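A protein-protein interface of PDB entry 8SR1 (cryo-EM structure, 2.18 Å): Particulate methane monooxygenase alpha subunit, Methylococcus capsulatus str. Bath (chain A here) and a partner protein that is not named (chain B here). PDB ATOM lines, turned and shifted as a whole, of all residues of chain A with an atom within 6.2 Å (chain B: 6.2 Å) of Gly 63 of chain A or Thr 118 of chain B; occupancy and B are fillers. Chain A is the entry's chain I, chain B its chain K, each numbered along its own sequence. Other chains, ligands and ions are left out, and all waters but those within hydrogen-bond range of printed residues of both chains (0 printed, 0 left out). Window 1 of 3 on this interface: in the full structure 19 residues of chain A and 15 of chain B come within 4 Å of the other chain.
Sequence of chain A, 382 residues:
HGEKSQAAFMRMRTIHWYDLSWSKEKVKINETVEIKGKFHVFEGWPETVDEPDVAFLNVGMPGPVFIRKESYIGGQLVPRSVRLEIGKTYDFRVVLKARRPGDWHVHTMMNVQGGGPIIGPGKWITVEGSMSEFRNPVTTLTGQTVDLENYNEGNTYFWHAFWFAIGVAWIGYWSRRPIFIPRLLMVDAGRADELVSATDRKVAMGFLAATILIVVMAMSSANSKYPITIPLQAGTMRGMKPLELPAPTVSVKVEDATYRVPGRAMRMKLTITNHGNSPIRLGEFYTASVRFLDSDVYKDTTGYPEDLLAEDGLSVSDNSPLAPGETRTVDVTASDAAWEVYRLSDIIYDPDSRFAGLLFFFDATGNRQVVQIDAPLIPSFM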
ATOM      1  N   MET A  61      -3.964 -10.735  -5.576  1.00  0.00           N
ATOM      2  CA  MET A  61      -4.426 -11.145  -6.892  1.00  0.00           C
ATOM      3  C   MET A  61      -5.035 -12.534  -6.787  1.00  0.00           C
ATOM      4  O   MET A  61      -4.704 -13.294  -5.865  1.00  0.00           O
ATOM      5  CB  MET A  61      -3.273 -11.124  -7.901  1.00  0.00           C
ATOM      6  CG  MET A  61      -2.428 -12.375  -7.906  1.00  0.00           C
ATOM      7  SD  MET A  61      -0.825 -12.110  -8.679  1.00  0.00           S
ATOM      8  CE  MET A  61      -1.215 -10.720  -9.728  1.00  0.00           C
ATOM      9  N   PRO A  62      -5.935 -12.896  -7.704  1.00  0.00           N
ATOM     10  CA  PRO A  62      -6.573 -14.218  -7.638  1.00  0.00           C
ATOM     11  C   PRO A  62      -5.719 -15.321  -8.240  1.00  0.00           C
ATOM     12  O   PRO A  62      -5.999 -15.792  -9.347  1.00  0.00           O
ATOM     13  CB  PRO A  62      -7.871 -14.030  -8.438  1.00  0.00           C
ATOM     14  CG  PRO A  62      -7.936 -12.575  -8.795  1.00  0.00           C
ATOM     15  CD  PRO A  62      -6.553 -12.044  -8.727  1.00  0.00           C
ATOM     16  N   GLY A  63      -4.679 -15.744  -7.527  1.00  0.00           N
ATOM     17  CA  GLY A  63      -3.777 -16.744  -8.041  1.00  0.00           C
ATOM     18  C   GLY A  63      -2.836 -16.155  -9.069  1.00  0.00           C
ATOM     19  O   GLY A  63      -2.898 -14.966  -9.387  1.00  0.00           O
ATOM     20  N   PRO A  64      -1.965 -16.981  -9.636  1.00  0.00           N
ATOM     21  CA  PRO A  64      -0.904 -16.468 -10.522  1.00  0.00           C
ATOM     22  C   PRO A  64      -1.428 -16.032 -11.892  1.00  0.00           C
ATOM     23  O   PRO A  64      -0.989 -16.521 -12.935  1.00  0.00           O
ATOM     24  CB  PRO A  64       0.056 -17.661 -10.620  1.00  0.00           C
ATOM     25  CG  PRO A  64      -0.539 -18.771  -9.801  1.00  0.00           C
ATOM     26  CD  PRO A  64      -1.962 -18.448  -9.577  1.00  0.00           C
ATOM     27  N   VAL A  65      -2.377 -15.096 -11.890  1.00  0.00           N
ATOM     28  CA  VAL A  65      -2.762 -14.450 -13.140  1.00  0.00           C
ATOM     29  C   VAL A  65      -1.652 -13.537 -13.642  1.00  0.00           C
ATOM     30  O   VAL A  65      -1.592 -13.240 -14.843  1.00  0.00           O
ATOM     31  CB  VAL A  65      -4.080 -13.672 -12.983  1.00  0.00           C
ATOM     32  CG1 VAL A  65      -5.185 -14.599 -12.502  1.00  0.00           C
ATOM     33  CG2 VAL A  65      -3.906 -12.497 -12.035  1.00  0.00           C
ATOM     34  N   PHE A  66      -0.778 -13.083 -12.747  1.00  0.00           N
ATOM     35  CA  PHE A  66       0.497 -12.473 -13.089  1.00  0.00           C
ATOM     36  C   PHE A  66       1.566 -13.263 -12.349  1.00  0.00           C
ATOM     37  O   PHE A  66       1.269 -13.903 -11.336  1.00  0.00           O
ATOM     38  CB  PHE A  66       0.573 -11.003 -12.663  1.00  0.00           C
ATOM     39  CG  PHE A  66      -0.296 -10.079 -13.463  1.00  0.00           C
ATOM     40  CD1 PHE A  66      -1.606  -9.843 -13.089  1.00  0.00           C
ATOM     41  CD2 PHE A  66       0.204  -9.424 -14.573  1.00  0.00           C
ATOM     42  CE1 PHE A  66      -2.406  -8.985 -13.815  1.00  0.00           C
ATOM     43  CE2 PHE A  66      -0.589  -8.564 -15.302  1.00  0.00           C
ATOM     44  CZ  PHE A  66      -1.894  -8.343 -14.918  1.00  0.00           C
ATOM     45  N   ARG A  99       0.078 -13.499 -17.252  1.00  0.00           N
ATOM     46  CA  ARG A  99       0.073 -14.943 -17.456  1.00  0.00           C
ATOM     47  C   ARG A  99      -1.289 -15.492 -17.854  1.00  0.00           C
ATOM     48  O   ARG A  99      -1.358 -16.408 -18.674  1.00  0.00           O
ATOM     49  CB  ARG A  99       0.561 -15.638 -16.173  1.00  0.00           C
ATOM     50  CG  ARG A  99       0.706 -17.142 -16.288  1.00  0.00           C
ATOM     51  CD  ARG A  99       1.327 -17.719 -15.030  1.00  0.00           C
ATOM     52  NE  ARG A  99       1.327 -19.177 -15.033  1.00  0.00           N
ATOM     53  CZ  ARG A  99       0.474 -19.924 -14.346  1.00  0.00           C
ATOM     54  NH1 ARG A  99      -0.471 -19.384 -13.595  1.00  0.00           N
ATOM     55  NH2 ARG A  99       0.575 -21.250 -14.414  1.00  0.00           N
ATOM     56  N   ARG A 100      -2.373 -14.949 -17.304  1.00  0.00           N
ATOM     57  CA  ARG A 100      -3.705 -15.476 -17.528  1.00  0.00           C
ATOM     58  C   ARG A 100      -4.630 -14.377 -18.034  1.00  0.00           C
ATOM     59  O   ARG A 100      -4.710 -13.308 -17.416  1.00  0.00           O
ATOM     60  CB  ARG A 100      -4.273 -16.079 -16.235  1.00  0.00           C
ATOM     61  CG  ARG A 100      -4.006 -17.566 -16.077  1.00  0.00           C
ATOM     62  CD  ARG A 100      -4.783 -18.134 -14.904  1.00  0.00           C
ATOM     63  NE  ARG A 100      -6.196 -18.298 -15.226  1.00  0.00           N
ATOM     64  CZ  ARG A 100      -7.184 -18.125 -14.358  1.00  0.00           C
ATOM     65  NH1 ARG A 100      -6.950 -17.793 -13.102  1.00  0.00           N
ATOM     66  NH2 ARG A 100      -8.440 -18.293 -14.766  1.00  0.00           N
ATOM     67  N   TRP B  30     -13.892 -16.932  -8.754  1.00  0.00           N
ATOM     68  CA  TRP B  30     -13.730 -15.533  -9.103  1.00  0.00           C
ATOM     69  C   TRP B  30     -15.041 -15.049  -9.698  1.00  0.00           C
ATOM     70  O   TRP B  30     -15.926 -15.856 -10.001  1.00  0.00           O
ATOM     71  CB  TRP B  30     -12.597 -15.358 -10.113  1.00  0.00           C
ATOM     72  CG  TRP B  30     -11.495 -16.341  -9.925  1.00  0.00           C
ATOM     73  CD1 TRP B  30     -10.358 -16.170  -9.197  1.00  0.00           C
ATOM     74  CD2 TRP B  30     -11.432 -17.663 -10.468  1.00  0.00           C
ATOM     75  NE1 TRP B  30      -9.584 -17.302  -9.257  1.00  0.00           N
ATOM     76  CE2 TRP B  30     -10.223 -18.234 -10.031  1.00  0.00           C
ATOM     77  CE3 TRP B  30     -12.282 -18.417 -11.282  1.00  0.00           C
ATOM     78  CZ2 TRP B  30      -9.842 -19.525 -10.381  1.00  0.00           C
ATOM     79  CZ3 TRP B  30     -11.903 -19.698 -11.628  1.00  0.00           C
ATOM     80  CH2 TRP B  30     -10.694 -20.236 -11.178  1.00  0.00           C
ATOM     81  N   GLY B 113      -7.427 -25.428   1.241  1.00  0.00           N
ATOM     82  CA  GLY B 113      -6.019 -25.007   1.174  1.00  0.00           C
ATOM     83  C   GLY B 113      -5.766 -24.190  -0.074  1.00  0.00           C
ATOM     84  O   GLY B 113      -5.437 -23.001   0.066  1.00  0.00           O
ATOM     85  N   THR B 114      -5.920 -24.813  -1.239  1.00  0.00           N
ATOM     86  CA  THR B 114      -5.667 -24.100  -2.515  1.00  0.00           C
ATOM     87  C   THR B 114      -6.426 -22.777  -2.479  1.00  0.00           C
ATOM     88  O   THR B 114      -5.960 -21.820  -3.106  1.00  0.00           O
ATOM     89  CB  THR B 114      -6.088 -24.936  -3.734  1.00  0.00           C
ATOM     90  OG1 THR B 114      -5.416 -24.416  -4.880  1.00  0.00           O
ATOM     91  CG2 THR B 114      -7.578 -24.923  -3.992  1.00  0.00           C
ATOM     92  N   TRP B 115      -7.532 -22.719  -1.741  1.00  0.00           N
ATOM     93  CA  TRP B 115      -8.319 -21.462  -1.839  1.00  0.00           C
ATOM     94  C   TRP B 115      -7.761 -20.452  -0.827  1.00  0.00           C
ATOM     95  O   TRP B 115      -7.294 -19.386  -1.268  1.00  0.00           O
ATOM     96  CB  TRP B 115      -9.802 -21.765  -1.604  1.00  0.00           C
ATOM     97  CG  TRP B 115     -10.641 -20.571  -1.261  1.00  0.00           C
ATOM     98  CD1 TRP B 115     -10.880 -20.066  -0.016  1.00  0.00           C
ATOM     99  CD2 TRP B 115     -11.380 -19.746  -2.177  1.00  0.00           C
ATOM    100  NE1 TRP B 115     -11.707 -18.979  -0.096  1.00  0.00           N
ATOM    101  CE2 TRP B 115     -12.029 -18.759  -1.408  1.00  0.00           C
ATOM    102  CE3 TRP B 115     -11.550 -19.741  -3.565  1.00  0.00           C
ATOM    103  CZ2 TRP B 115     -12.833 -17.777  -1.985  1.00  0.00           C
ATOM    104  CZ3 TRP B 115     -12.346 -18.771  -4.135  1.00  0.00           C
ATOM    105  CH2 TRP B 115     -12.976 -17.804  -3.352  1.00  0.00           C
ATOM    106  N   HIS B 116      -7.772 -20.789   0.473  1.00  0.00           N
ATOM    107  CA  HIS B 116      -7.321 -19.826   1.517  1.00  0.00           C
ATOM    108  C   HIS B 116      -5.857 -19.419   1.287  1.00  0.00           C
ATOM    109  O   HIS B 116      -5.495 -18.305   1.691  1.00  0.00           O
ATOM    110  CB  HIS B 116      -7.481 -20.380   2.918  1.00  0.00           C
ATOM    111  CG  HIS B 116      -8.938 -20.482   3.143  1.00  0.00           C
ATOM    112  ND1 HIS B 116      -9.818 -19.482   2.819  1.00  0.00           N
ATOM    113  CD2 HIS B 116      -9.642 -21.571   3.500  1.00  0.00           C
ATOM    114  CE1 HIS B 116     -11.046 -19.911   3.062  1.00  0.00           C
ATOM    115  NE2 HIS B 116     -10.950 -21.207   3.450  1.00  0.00           N
ATOM    116  N   GLN B 117      -5.041 -20.275   0.664  1.00  0.00           N
ATOM    117  CA  GLN B 117      -3.589 -19.954   0.550  1.00  0.00           C
ATOM    118  C   GLN B 117      -3.281 -19.160  -0.728  1.00  0.00           C
ATOM    119  O   GLN B 117      -2.082 -18.950  -1.003  1.00  0.00           O
ATOM    120  CB  GLN B 117      -2.761 -21.239   0.609  1.00  0.00           C
ATOM    121  CG  GLN B 117      -2.942 -22.012   1.907  1.00  0.00           C
ATOM    122  CD  GLN B 117      -1.937 -21.629   2.965  1.00  0.00           C
ATOM    123  OE1 GLN B 117      -1.440 -22.471   3.708  1.00  0.00           O
ATOM    124  NE2 GLN B 117      -1.632 -20.344   3.046  1.00  0.00           N
ATOM    125  N   THR B 118      -4.307 -18.725  -1.466  1.00  0.00           N
ATOM    126  CA  THR B 118      -4.075 -18.013  -2.753  1.00  0.00           C
ATOM    127  C   THR B 118      -5.001 -16.798  -2.840  1.00  0.00           C
ATOM    128  O   THR B 118      -4.638 -15.831  -3.533  1.00  0.00           O
ATOM    129  CB  THR B 118      -4.296 -18.960  -3.939  1.00  0.00           C
ATOM    130  OG1 THR B 118      -5.690 -19.262  -3.997  1.00  0.00           O
ATOM    131  CG2 THR B 118      -3.498 -20.239  -3.819  1.00  0.00           C
ATOM    132  N   ILE B 119      -6.159 -16.865  -2.183  1.00  0.00           N
ATOM    133  CA  ILE B 119      -7.143 -15.736  -2.167  1.00  0.00           C
ATOM    134  C   ILE B 119      -6.808 -14.814  -0.989  1.00  0.00           C
ATOM    135  O   ILE B 119      -6.121 -15.278  -0.059  1.00  0.00           O
ATOM    136  CB  ILE B 119      -8.600 -16.234  -2.111  1.00  0.00           C
ATOM    137  CG1 ILE B 119      -8.926 -16.879  -0.760  1.00  0.00           C
ATOM    138  CG2 ILE B 119      -8.898 -17.173  -3.270  1.00  0.00           C
ATOM    139  CD1 ILE B 119     -10.083 -16.235  -0.034  1.00  0.00           C
ATOM    140  N   VAL B 120      -7.296 -13.575  -1.021  1.00  0.00           N
ATOM    141  CA  VAL B 120      -6.940 -12.578   0.031  1.00  0.00           C
ATOM    142  C   VAL B 120      -7.831 -12.781   1.254  1.00  0.00           C
ATOM    143  O   VAL B 120      -7.692 -11.978   2.192  1.00  0.00           O
ATOM    144  CB  VAL B 120      -7.045 -11.138  -0.506  1.00  0.00           C
ATOM    145  CG1 VAL B 120      -5.946 -10.250   0.053  1.00  0.00           C
ATOM    146  CG2 VAL B 120      -7.046 -11.101  -2.026  1.00  0.00           C
ATOM    147  N   ARG B 121      -8.701 -13.796   1.246  1.00  0.00           N
ATOM    148  CA  ARG B 121      -9.523 -14.139   2.445  1.00  0.00           C
ATOM    149  C   ARG B 121     -10.524 -13.002   2.736  1.00  0.00           C
ATOM    150  O   ARG B 121     -10.279 -11.881   2.251  1.00  0.00           O
ATOM    151  CB  ARG B 121      -8.558 -14.515   3.577  1.00  0.00           C
ATOM    152  CG  ARG B 121      -7.066 -14.510   3.245  1.00  0.00           C
ATOM    153  CD  ARG B 121      -6.533 -15.835   2.809  1.00  0.00           C
ATOM    154  NE  ARG B 121      -6.866 -17.105   3.452  1.00  0.00           N
ATOM    155  CZ  ARG B 121      -7.587 -17.288   4.524  1.00  0.00           C
ATOM    156  NH1 ARG B 121      -7.043 -17.805   5.611  1.00  0.00           N
ATOM    157  NH2 ARG B 121      -8.884 -17.037   4.506  1.00  0.00           N
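The backbone carbonyl oxygen (O) of Met 61 of chain A sits close to the backbone carbonyl oxygen (O) of Thr 118 of chain B, 3.4 Å away.
OG1 of Thr 118 of chain B is in hydrogen-bond range of O of Thr 114 of chain B (2.7 Å). O of Trp 115 of chain B is in hydrogen-bond range of OG1 of Thr 118 of chain B, at 3.2 Å.
Trp 30 of chain B touches Pro 62 of chain A. Thr 118 of chain B touches Gly 63 of chain A (O to N, 3.995 Å).
Of the printed residues of chain B, Met 61 of chain A touches Thr 118. Printed residues of chain B within 4 Å of Pro 62 of chain A: Trp 30 (3.4 Å). Of the printed residues of chain B, Gly 63 of chain A touches Thr 118. Printed residues of chain A within 4 Å of Trp 30 of chain B: Pro 62 (3.4 Å). Of the printed residues of chain A, Thr 118 of chain B touches Met 61 (3.4 Å) and Gly 63 (3.995 Å). Ile 119 of chain B touches none of the printed residues of chain A. The nearest printed residue of chain A that does not touch Thr 118 of chain B is Pro 62 of chain A (4.8 Å). The nearest printed residue of chain B that does not touch Met 61 of chain A is Val 120 of chain B (4.7 Å).
Printed residues of chain A that touch a printed residue of chain B: Met 61, Pro 62 and Gly 63. Hydrophobic or aromatic side chains of chain A within 4 Å of the printed part of chain B: Pro 62. Along chain A the printed residues that touch a printed residue of chain B span positions 61 to 63. Printed residues of chain B that touch a printed residue of chain A: Trp 30 and Thr 118. Hydrophobic or aromatic side chains of chain B that line the printed part of chain A: Trp 30. Among the printed residues, no Asp or Glu carboxylate lies within 4 Å of a Lys or Arg side-chain nitrogen of the other chain.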
